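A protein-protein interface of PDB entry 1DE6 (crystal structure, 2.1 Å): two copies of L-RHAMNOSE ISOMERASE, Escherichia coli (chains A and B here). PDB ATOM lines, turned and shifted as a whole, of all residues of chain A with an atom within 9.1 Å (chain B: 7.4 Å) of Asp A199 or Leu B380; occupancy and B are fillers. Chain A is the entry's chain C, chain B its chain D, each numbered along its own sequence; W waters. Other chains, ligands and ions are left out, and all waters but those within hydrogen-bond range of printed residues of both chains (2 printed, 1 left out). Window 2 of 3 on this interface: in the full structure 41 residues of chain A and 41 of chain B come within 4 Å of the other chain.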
ATOM      1  N   PHE A 152      -6.128  12.144 -22.394  1.00  0.00           N
ATOM      2  CA  PHE A 152      -7.084  11.025 -22.611  1.00  0.00           C
ATOM      3  C   PHE A 152      -7.590  11.107 -24.026  1.00  0.00           C
ATOM      4  O   PHE A 152      -7.737  12.194 -24.582  1.00  0.00           O
ATOM      5  CB  PHE A 152      -8.310  10.997 -21.632  1.00  0.00           C
ATOM      6  CG  PHE A 152      -7.765  10.910 -20.229  1.00  0.00           C
ATOM      7  CD1 PHE A 152      -7.394   9.670 -19.713  1.00  0.00           C
ATOM      8  CD2 PHE A 152      -7.541  12.049 -19.452  1.00  0.00           C
ATOM      9  CE1 PHE A 152      -6.820   9.569 -18.446  1.00  0.00           C
ATOM     10  CE2 PHE A 152      -6.975  11.965 -18.181  1.00  0.00           C
ATOM     11  CZ  PHE A 152      -6.603  10.721 -17.691  1.00  0.00           C
ATOM     12  N   GLY A 196      -3.366   8.222 -19.725  1.00  0.00           N
ATOM     13  CA  GLY A 196      -2.870   7.944 -18.366  1.00  0.00           C
ATOM     14  C   GLY A 196      -2.808   9.151 -17.401  1.00  0.00           C
ATOM     15  O   GLY A 196      -3.246  10.285 -17.696  1.00  0.00           O
ATOM     16  N   MET A 197      -2.215   8.915 -16.220  1.00  0.00           N
ATOM     17  CA  MET A 197      -2.088   9.962 -15.225  1.00  0.00           C
ATOM     18  C   MET A 197      -0.691  10.184 -14.763  1.00  0.00           C
ATOM     19  O   MET A 197       0.084   9.267 -14.628  1.00  0.00           O
ATOM     20  CB  MET A 197      -2.917   9.749 -13.958  1.00  0.00           C
ATOM     21  CG  MET A 197      -4.391   9.946 -14.217  1.00  0.00           C
ATOM     22  SD  MET A 197      -5.015  11.594 -13.869  1.00  0.00           S
ATOM     23  CE  MET A 197      -6.772  11.107 -13.938  1.00  0.00           C
ATOM     24  N   LYS A 198      -0.426  11.457 -14.516  1.00  0.00           N
ATOM     25  CA  LYS A 198       0.894  11.781 -14.057  1.00  0.00           C
ATOM     26  C   LYS A 198       1.104  11.265 -12.655  1.00  0.00           C
ATOM     27  O   LYS A 198       2.019  10.467 -12.417  1.00  0.00           O
ATOM     28  CB  LYS A 198       1.172  13.215 -14.216  1.00  0.00           C
ATOM     29  CG  LYS A 198       2.308  13.618 -13.304  1.00  0.00           C
ATOM     30  CD  LYS A 198       3.030  14.886 -13.705  1.00  0.00           C
ATOM     31  CE  LYS A 198       4.281  15.203 -12.870  1.00  0.00           C
ATOM     32  NZ  LYS A 198       4.744  16.607 -13.030  1.00  0.00           N
ATOM     33  N   ASP A 199       0.140  11.606 -11.775  1.00  0.00           N
ATOM     34  CA  ASP A 199       0.191  11.333 -10.352  1.00  0.00           C
ATOM     35  C   ASP A 199      -0.751  10.316  -9.758  1.00  0.00           C
ATOM     36  O   ASP A 199      -1.521   9.648 -10.484  1.00  0.00           O
ATOM     37  CB  ASP A 199       0.279  12.679  -9.589  1.00  0.00           C
ATOM     38  CG  ASP A 199       1.224  12.608  -8.409  1.00  0.00           C
ATOM     39  OD1 ASP A 199       1.640  11.571  -7.933  1.00  0.00           O
ATOM     40  OD2 ASP A 199       1.633  13.784  -7.964  1.00  0.00           O
ATOM     41  N   ILE A 200      -0.639  10.159  -8.427  1.00  0.00           N
ATOM     42  CA  ILE A 200      -1.483   9.180  -7.722  1.00  0.00           C
ATOM     43  C   ILE A 200      -2.939   9.297  -8.201  1.00  0.00           C
ATOM     44  O   ILE A 200      -3.535  10.382  -8.172  1.00  0.00           O
ATOM     45  CB  ILE A 200      -1.462   9.404  -6.228  1.00  0.00           C
ATOM     46  CG1 ILE A 200      -0.030   9.490  -5.710  1.00  0.00           C
ATOM     47  CG2 ILE A 200      -2.124   8.149  -5.690  1.00  0.00           C
ATOM     48  CD1 ILE A 200       0.813   8.341  -6.266  1.00  0.00           C
ATOM     49  N   THR A 201      -3.485   8.196  -8.680  1.00  0.00           N
ATOM     50  CA  THR A 201      -4.816   8.117  -9.241  1.00  0.00           C
ATOM     51  C   THR A 201      -5.845   7.466  -8.334  1.00  0.00           C
ATOM     52  O   THR A 201      -5.576   6.435  -7.680  1.00  0.00           O
ATOM     53  CB  THR A 201      -4.672   7.265 -10.478  1.00  0.00           C
ATOM     54  OG1 THR A 201      -3.742   7.941 -11.349  1.00  0.00           O
ATOM     55  CG2 THR A 201      -6.010   6.994 -11.127  1.00  0.00           C
ATOM     56  N   VAL A 202      -7.030   8.085  -8.287  1.00  0.00           N
ATOM     57  CA  VAL A 202      -8.168   7.558  -7.496  1.00  0.00           C
ATOM     58  C   VAL A 202      -8.905   6.449  -8.270  1.00  0.00           C
ATOM     59  O   VAL A 202      -9.153   5.324  -7.759  1.00  0.00           O
ATOM     60  CB  VAL A 202      -9.162   8.684  -7.240  1.00  0.00           C
ATOM     61  CG1 VAL A 202     -10.353   8.100  -6.514  1.00  0.00           C
ATOM     62  CG2 VAL A 202      -8.479   9.758  -6.414  1.00  0.00           C
ATOM     63  N   ASP A 203      -9.201   6.720  -9.553  1.00  0.00           N
ATOM     64  CA  ASP A 203      -9.920   5.696 -10.281  1.00  0.00           C
ATOM     65  C   ASP A 203      -9.271   5.179 -11.536  1.00  0.00           C
ATOM     66  O   ASP A 203      -9.432   5.757 -12.643  1.00  0.00           O
ATOM     67  CB  ASP A 203     -11.357   6.171 -10.616  1.00  0.00           C
ATOM     68  CG  ASP A 203     -12.268   5.084 -11.266  1.00  0.00           C
ATOM     69  OD1 ASP A 203     -11.955   3.905 -11.571  1.00  0.00           O
ATOM     70  OD2 ASP A 203     -13.470   5.541 -11.517  1.00  0.00           O
ATOM     71  N   ARG A 204      -8.628   4.003 -11.414  1.00  0.00           N
ATOM     72  CA  ARG A 204      -8.012   3.448 -12.596  1.00  0.00           C
ATOM     73  C   ARG A 204      -9.006   2.624 -13.341  1.00  0.00           C
ATOM     74  O   ARG A 204      -8.687   2.218 -14.440  1.00  0.00           O
ATOM     75  CB  ARG A 204      -6.839   2.519 -12.235  1.00  0.00           C
ATOM     76  CG  ARG A 204      -5.740   3.348 -11.580  1.00  0.00           C
ATOM     77  CD  ARG A 204      -4.874   2.728 -10.518  1.00  0.00           C
ATOM     78  NE  ARG A 204      -3.607   2.462 -11.064  1.00  0.00           N
ATOM     79  CZ  ARG A 204      -2.389   3.015 -10.986  1.00  0.00           C
ATOM     80  NH1 ARG A 204      -1.935   4.059 -10.222  1.00  0.00           N
ATOM     81  NH2 ARG A 204      -1.578   2.334 -11.831  1.00  0.00           N
ATOM     82  N   GLY A 238       4.710   6.855 -19.360  1.00  0.00           N
ATOM     83  CA  GLY A 238       5.218   7.903 -20.252  1.00  0.00           C
ATOM     84  C   GLY A 238       5.552   9.152 -19.482  1.00  0.00           C
ATOM     85  O   GLY A 238       5.000   9.306 -18.407  1.00  0.00           O
ATOM     86  N   GLY A 240       5.182  12.534 -17.990  1.00  0.00           N
ATOM     87  CA  GLY A 240       3.922  13.303 -17.855  1.00  0.00           C
ATOM     88  C   GLY A 240       2.696  12.368 -17.637  1.00  0.00           C
ATOM     89  O   GLY A 240       1.577  12.794 -17.553  1.00  0.00           O
ATOM     90  N   ALA A 241       2.915  11.077 -17.545  1.00  0.00           N
ATOM     91  CA  ALA A 241       1.838  10.137 -17.249  1.00  0.00           C
ATOM     92  C   ALA A 241       2.524   8.990 -16.536  1.00  0.00           C
ATOM     93  O   ALA A 241       2.382   7.840 -16.881  1.00  0.00           O
ATOM     94  CB  ALA A 241       1.227   9.620 -18.537  1.00  0.00           C
ATOM     95  N   GLU A 242       3.387   9.305 -15.568  1.00  0.00           N
ATOM     96  CA  GLU A 242       4.174   8.297 -14.881  1.00  0.00           C
ATOM     97  C   GLU A 242       3.408   7.317 -14.008  1.00  0.00           C
ATOM     98  O   GLU A 242       3.828   6.188 -13.902  1.00  0.00           O
ATOM     99  CB  GLU A 242       5.250   8.927 -13.934  1.00  0.00           C
ATOM    100  CG  GLU A 242       6.378   9.650 -14.702  1.00  0.00           C
ATOM    101  CD  GLU A 242       6.005  11.028 -15.223  1.00  0.00           C
ATOM    102  OE1 GLU A 242       6.833  11.718 -15.778  1.00  0.00           O
ATOM    103  OE2 GLU A 242       4.773  11.461 -14.973  1.00  0.00           O
ATOM    104  N   SER A 243       2.341   7.747 -13.315  1.00  0.00           N
ATOM    105  CA  SER A 243       1.709   6.875 -12.390  1.00  0.00           C
ATOM    106  C   SER A 243       0.810   5.814 -12.874  1.00  0.00           C
ATOM    107  O   SER A 243       0.630   4.803 -12.180  1.00  0.00           O
ATOM    108  CB  SER A 243       0.966   7.689 -11.366  1.00  0.00           C
ATOM    109  OG  SER A 243       1.842   8.525 -10.727  1.00  0.00           O
ATOM    110  N   TYR A 244       0.162   6.082 -13.978  1.00  0.00           N
ATOM    111  CA  TYR A 244      -0.861   5.118 -14.439  1.00  0.00           C
ATOM    112  C   TYR A 244      -1.102   5.271 -15.902  1.00  0.00           C
ATOM    113  O   TYR A 244      -1.193   6.423 -16.381  1.00  0.00           O
ATOM    114  CB  TYR A 244      -2.188   5.594 -13.735  1.00  0.00           C
ATOM    115  CG  TYR A 244      -3.507   5.136 -14.365  1.00  0.00           C
ATOM    116  CD1 TYR A 244      -3.837   3.790 -14.510  1.00  0.00           C
ATOM    117  CD2 TYR A 244      -4.443   6.090 -14.776  1.00  0.00           C
ATOM    118  CE1 TYR A 244      -5.058   3.404 -15.067  1.00  0.00           C
ATOM    119  CE2 TYR A 244      -5.686   5.729 -15.303  1.00  0.00           C
ATOM    120  CZ  TYR A 244      -6.002   4.374 -15.434  1.00  0.00           C
ATOM    121  OH  TYR A 244      -7.234   4.045 -15.984  1.00  0.00           O
ATOM    122  N   THR A 245      -1.260   4.148 -16.554  1.00  0.00           N
ATOM    123  CA  THR A 245      -1.579   4.047 -17.982  1.00  0.00           C
ATOM    124  C   THR A 245      -2.823   3.197 -18.098  1.00  0.00           C
ATOM    125  O   THR A 245      -2.874   2.049 -17.585  1.00  0.00           O
ATOM    126  CB  THR A 245      -0.456   3.296 -18.783  1.00  0.00           C
ATOM    127  OG1 THR A 245       0.802   3.948 -18.634  1.00  0.00           O
ATOM    128  CG2 THR A 245      -0.743   3.116 -20.288  1.00  0.00           C
ATOM    129  N   LEU B 367     -13.108  12.436  -3.860  1.00  0.00           N
ATOM    130  CA  LEU B 367     -11.845  12.300  -4.580  1.00  0.00           C
ATOM    131  C   LEU B 367     -12.046  11.920  -6.020  1.00  0.00           C
ATOM    132  O   LEU B 367     -11.355  12.461  -6.918  1.00  0.00           O
ATOM    133  CB  LEU B 367     -10.914  11.306  -3.922  1.00  0.00           C
ATOM    134  CG  LEU B 367     -10.403  11.822  -2.600  1.00  0.00           C
ATOM    135  CD1 LEU B 367      -9.710  10.641  -1.925  1.00  0.00           C
ATOM    136  CD2 LEU B 367      -9.402  12.935  -2.834  1.00  0.00           C
ATOM    137  N   LEU B 370     -13.253  14.957  -7.575  1.00  0.00           N
ATOM    138  CA  LEU B 370     -12.195  15.931  -7.887  1.00  0.00           C
ATOM    139  C   LEU B 370     -11.344  15.570  -9.106  1.00  0.00           C
ATOM    140  O   LEU B 370     -11.014  16.412  -9.957  1.00  0.00           O
ATOM    141  CB  LEU B 370     -11.288  16.065  -6.709  1.00  0.00           C
ATOM    142  CG  LEU B 370     -11.919  16.800  -5.530  1.00  0.00           C
ATOM    143  CD1 LEU B 370     -11.106  16.563  -4.257  1.00  0.00           C
ATOM    144  CD2 LEU B 370     -11.831  18.293  -5.861  1.00  0.00           C
ATOM    145  N   GLU B 371     -10.996  14.273  -9.177  1.00  0.00           N
ATOM    146  CA  GLU B 371     -10.221  13.738 -10.280  1.00  0.00           C
ATOM    147  C   GLU B 371     -10.898  13.941 -11.660  1.00  0.00           C
ATOM    148  O   GLU B 371     -10.289  14.344 -12.682  1.00  0.00           O
ATOM    149  CB  GLU B 371      -9.941  12.257 -10.027  1.00  0.00           C
ATOM    150  CG  GLU B 371      -9.075  11.614 -11.140  1.00  0.00           C
ATOM    151  CD  GLU B 371      -8.596  10.262 -10.663  1.00  0.00           C
ATOM    152  OE1 GLU B 371      -9.288   9.260 -10.718  1.00  0.00           O
ATOM    153  OE2 GLU B 371      -7.419  10.283 -10.088  1.00  0.00           O
ATOM    154  N   ASP B 375      -9.190  18.363 -10.947  1.00  0.00           N
ATOM    155  CA  ASP B 375      -8.679  19.037  -9.731  1.00  0.00           C
ATOM    156  C   ASP B 375      -7.586  18.143  -8.998  1.00  0.00           C
ATOM    157  O   ASP B 375      -7.807  17.563  -7.914  1.00  0.00           O
ATOM    158  CB  ASP B 375      -9.768  19.520  -8.708  1.00  0.00           C
ATOM    159  CG  ASP B 375      -9.114  20.456  -7.704  1.00  0.00           C
ATOM    160  OD1 ASP B 375      -7.911  20.635  -7.590  1.00  0.00           O
ATOM    161  OD2 ASP B 375      -9.931  21.127  -6.977  1.00  0.00           O
ATOM    162  N   TYR B 376      -6.423  18.006  -9.678  1.00  0.00           N
ATOM    163  CA  TYR B 376      -5.264  17.228  -9.319  1.00  0.00           C
ATOM    164  C   TYR B 376      -4.583  17.715  -8.128  1.00  0.00           C
ATOM    165  O   TYR B 376      -4.069  16.909  -7.356  1.00  0.00           O
ATOM    166  CB  TYR B 376      -4.298  17.113 -10.518  1.00  0.00           C
ATOM    167  CG  TYR B 376      -4.942  16.298 -11.645  1.00  0.00           C
ATOM    168  CD1 TYR B 376      -6.176  15.647 -11.510  1.00  0.00           C
ATOM    169  CD2 TYR B 376      -4.324  16.297 -12.896  1.00  0.00           C
ATOM    170  CE1 TYR B 376      -6.753  14.981 -12.593  1.00  0.00           C
ATOM    171  CE2 TYR B 376      -4.878  15.623 -13.977  1.00  0.00           C
ATOM    172  CZ  TYR B 376      -6.092  14.958 -13.826  1.00  0.00           C
ATOM    173  OH  TYR B 376      -6.580  14.303 -14.947  1.00  0.00           O
ATOM    174  N   THR B 377      -4.615  19.021  -7.961  1.00  0.00           N
ATOM    175  CA  THR B 377      -4.051  19.706  -6.810  1.00  0.00           C
ATOM    176  C   THR B 377      -4.842  19.209  -5.580  1.00  0.00           C
ATOM    177  O   THR B 377      -4.349  18.644  -4.604  1.00  0.00           O
ATOM    178  CB  THR B 377      -4.271  21.213  -6.935  1.00  0.00           C
ATOM    179  OG1 THR B 377      -3.638  21.756  -8.122  1.00  0.00           O
ATOM    180  CG2 THR B 377      -3.674  21.848  -5.717  1.00  0.00           C
ATOM    181  N   ALA B 378      -6.143  19.379  -5.618  1.00  0.00           N
ATOM    182  CA  ALA B 378      -6.953  18.979  -4.507  1.00  0.00           C
ATOM    183  C   ALA B 378      -6.894  17.463  -4.257  1.00  0.00           C
ATOM    184  O   ALA B 378      -6.845  16.985  -3.118  1.00  0.00           O
ATOM    185  CB  ALA B 378      -8.360  19.534  -4.614  1.00  0.00           C
ATOM    186  N   ARG B 379      -6.833  16.674  -5.296  1.00  0.00           N
ATOM    187  CA  ARG B 379      -6.737  15.251  -5.114  1.00  0.00           C
ATOM    188  C   ARG B 379      -5.471  14.816  -4.353  1.00  0.00           C
ATOM    189  O   ARG B 379      -5.393  14.045  -3.385  1.00  0.00           O
ATOM    190  CB  ARG B 379      -6.655  14.662  -6.516  1.00  0.00           C
ATOM    191  CG  ARG B 379      -6.418  13.149  -6.585  1.00  0.00           C
ATOM    192  CD  ARG B 379      -6.358  12.614  -8.041  1.00  0.00           C
ATOM    193  NE  ARG B 379      -5.130  13.096  -8.704  1.00  0.00           N
ATOM    194  CZ  ARG B 379      -4.751  12.801  -9.938  1.00  0.00           C
ATOM    195  NH1 ARG B 379      -5.476  11.984 -10.726  1.00  0.00           N
ATOM    196  NH2 ARG B 379      -3.597  13.327 -10.346  1.00  0.00           N
ATOM    197  N   LEU B 380      -4.384  15.395  -4.793  1.00  0.00           N
ATOM    198  CA  LEU B 380      -3.154  15.014  -4.149  1.00  0.00           C
ATOM    199  C   LEU B 380      -3.211  15.446  -2.731  1.00  0.00           C
ATOM    200  O   LEU B 380      -2.884  14.697  -1.791  1.00  0.00           O
ATOM    201  CB  LEU B 380      -1.867  15.636  -4.784  1.00  0.00           C
ATOM    202  CG  LEU B 380      -0.556  15.084  -4.134  1.00  0.00           C
ATOM    203  CD1 LEU B 380      -0.443  13.591  -4.287  1.00  0.00           C
ATOM    204  CD2 LEU B 380       0.635  15.700  -4.901  1.00  0.00           C
ATOM    205  N   ALA B 381      -3.617  16.700  -2.643  1.00  0.00           N
ATOM    206  CA  ALA B 381      -3.649  17.230  -1.345  1.00  0.00           C
ATOM    207  C   ALA B 381      -4.496  16.408  -0.420  1.00  0.00           C
ATOM    208  O   ALA B 381      -4.111  16.079   0.714  1.00  0.00           O
ATOM    209  CB  ALA B 381      -4.075  18.671  -1.359  1.00  0.00           C
ATOM    210  N   LEU B 382      -5.676  16.089  -0.901  1.00  0.00           N
ATOM    211  CA  LEU B 382      -6.561  15.326  -0.050  1.00  0.00           C
ATOM    212  C   LEU B 382      -6.094  13.941   0.121  1.00  0.00           C
ATOM    213  O   LEU B 382      -6.239  13.412   1.186  1.00  0.00           O
ATOM    214  CB  LEU B 382      -7.890  15.185  -0.723  1.00  0.00           C
ATOM    215  CG  LEU B 382      -8.763  16.329  -0.328  1.00  0.00           C
ATOM    216  CD1 LEU B 382      -9.784  15.744   0.636  1.00  0.00           C
ATOM    217  CD2 LEU B 382      -7.891  17.370   0.354  1.00  0.00           C
ATOM    218  N   LEU B 383      -5.599  13.333  -0.916  1.00  0.00           N
ATOM    219  CA  LEU B 383      -5.135  12.005  -0.653  1.00  0.00           C
ATOM    220  C   LEU B 383      -4.151  12.017   0.518  1.00  0.00           C
ATOM    221  O   LEU B 383      -4.148  11.137   1.358  1.00  0.00           O
ATOM    222  CB  LEU B 383      -4.302  11.480  -1.844  1.00  0.00           C
ATOM    223  CG  LEU B 383      -5.261  10.855  -2.831  1.00  0.00           C
ATOM    224  CD1 LEU B 383      -4.621  10.564  -4.177  1.00  0.00           C
ATOM    225  CD2 LEU B 383      -5.865   9.562  -2.274  1.00  0.00           C
ATOM    226  N   GLU B 384      -3.248  12.991   0.504  1.00  0.00           N
ATOM    227  CA  GLU B 384      -2.196  13.091   1.523  1.00  0.00           C
ATOM    228  C   GLU B 384      -2.701  13.389   2.921  1.00  0.00           C
ATOM    229  O   GLU B 384      -2.343  12.760   3.928  1.00  0.00           O
ATOM    230  CB  GLU B 384      -1.071  14.020   1.051  1.00  0.00           C
ATOM    231  CG  GLU B 384      -0.184  13.342  -0.005  1.00  0.00           C
ATOM    232  CD  GLU B 384       0.618  12.168   0.528  1.00  0.00           C
ATOM    233  OE1 GLU B 384       1.526  12.189   1.327  1.00  0.00           O
ATOM    234  OE2 GLU B 384       0.263  11.087  -0.008  1.00  0.00           O
ATOM    235  N   GLU B 385      -3.634  14.302   2.987  1.00  0.00           N
ATOM    236  CA  GLU B 385      -4.238  14.678   4.280  1.00  0.00           C
ATOM    237  C   GLU B 385      -4.888  13.497   4.999  1.00  0.00           C
ATOM    238  O   GLU B 385      -4.983  13.347   6.228  1.00  0.00           O
ATOM    239  CB  GLU B 385      -5.270  15.792   3.970  1.00  0.00           C
ATOM    240  CG  GLU B 385      -4.532  17.142   3.873  1.00  0.00           C
ATOM    241  CD  GLU B 385      -3.548  17.347   5.024  1.00  0.00           C
ATOM    242  OE1 GLU B 385      -3.784  17.161   6.220  1.00  0.00           O
ATOM    243  OE2 GLU B 385      -2.455  17.932   4.609  1.00  0.00           O
ATOM    244  N   GLN B 386      -5.353  12.626   4.187  1.00  0.00           N
ATOM    245  CA  GLN B 386      -6.020  11.453   4.657  1.00  0.00           C
ATOM    246  C   GLN B 386      -5.100  10.715   5.620  1.00  0.00           C
ATOM    247  O   GLN B 386      -5.518  10.126   6.617  1.00  0.00           O
ATOM    248  CB  GLN B 386      -6.429  10.665   3.401  1.00  0.00           C
ATOM    249  CG  GLN B 386      -7.264   9.458   3.639  1.00  0.00           C
ATOM    250  CD  GLN B 386      -8.649   9.822   4.133  1.00  0.00           C
ATOM    251  OE1 GLN B 386      -9.126  10.928   3.835  1.00  0.00           O
ATOM    252  NE2 GLN B 386      -9.290   8.894   4.910  1.00  0.00           N
HETATM  253  O   HOH W   1      -2.944  12.677  -6.901  1.00  0.00           O
HETATM  254  O   HOH W   2      -9.733   8.336 -13.267  1.00  0.00           O
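The backbone NH (N) of Asp A203 is in hydrogen-bond range of the side-chain carboxylate (OE1) of Glu B371 (2.8 Å).
O of Ile A200 lies within hydrogen-bond range of NE of Arg B379 (3.2 Å).
The side-chain sulfur (SD) of Met A197 sits at hydrogen-bond distance from the guanidinium group (NH1) of Arg B379.
The side-chain carboxylate of Glu B371 is in hydrogen-bond range of the backbone NH of Val A202, at 2.9 Å.
The side-chain sulfur (SD) of Met A197 sits at hydrogen-bond distance from the side-chain hydroxyl (OH) of Tyr B376, 3.3 Å away.
The backbone carbonyl oxygen (O) of Asp A199 sits at hydrogen-bond distance from the side-chain hydroxyl (OG1) of Thr A201, 2.9 Å away.
N of Glu A242 is in hydrogen-bond range of O of Met A197.
The guanidinium group (NH1) of Arg B379 is in salt-bridge range of the side-chain carboxylate (OE2) of Glu B371.
N of Met A197 sits at hydrogen-bond distance from O of Tyr A244 (2.7 Å).
O of Met A197 lies within hydrogen-bond range of N of Ser A243.
Glu B371 touches Met A197 (CG to CE, 3.7 Å).
OD2 of Asp A199 touches CD2 of Leu B380, 3.7 Å away.
Ile A200 touches Leu B383 (CG2 to CD1, 3.8 Å).
Thr A201 touches Glu B371.
Leu B367 touches Val A202 (CB to CG2, 3.8 Å).
Val A202 touches Arg B379 (CG2 to CD, 3.9 Å).
Of chain A, only Asp A199 (3.7 Å) comes within 4 Å of Leu B380.
No residue of chain A comes within 4 Å of Ala B381.
Printed residues of chain B within 4 Å of Thr A201: Glu B371.
Printed residues of chain B within 4 Å of Val A202: Leu B367, Glu B371 and Arg B379.
Of the printed residues of chain A, Leu B367 touches Val A202.
Of the printed residues of chain A, Leu B383 touches Ile A200 (3.8 Å).
Of the printed residues of chain A, Tyr B376 touches Met A197 (3.3 Å).
The nearest printed residue of chain B that does not touch Asp A199 is Arg B379 (4.002 Å).
The nearest residue of chain A that does not touch Leu B380 is Ile A200 (4.4 Å).
The nearest printed residue of chain A that does not touch Leu B367 is Asp A203 (6.7 Å).
Of the 17 printed residues of chain A, 6 touch a printed residue of chain B.
Printed residues of chain A that touch a printed residue of chain B: Met A197, Asp A199, Ile A200, Thr A201, Val A202 and Asp A203.
Among the printed residues, no Asp or Glu carboxylate lies within 4 Å of a Lys or Arg side-chain nitrogen of the other chain.
No position is printed for both chains.
Of the 11 pairs that touch across the chains among the printed residues, none has its exchanged pair printed and touching as well.
Water W2 bridges the backbone carbonyl oxygen (O) of Asp A203 (2.7 Å) and the side-chain carboxylate (OE1) of Glu B371 (2.7 Å).
Water W1 lies within hydrogen-bond range of the backbone carbonyl oxygen of Ile A200 (2.7 Å) and the guanidinium group of Arg B379 (2.9 Å).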
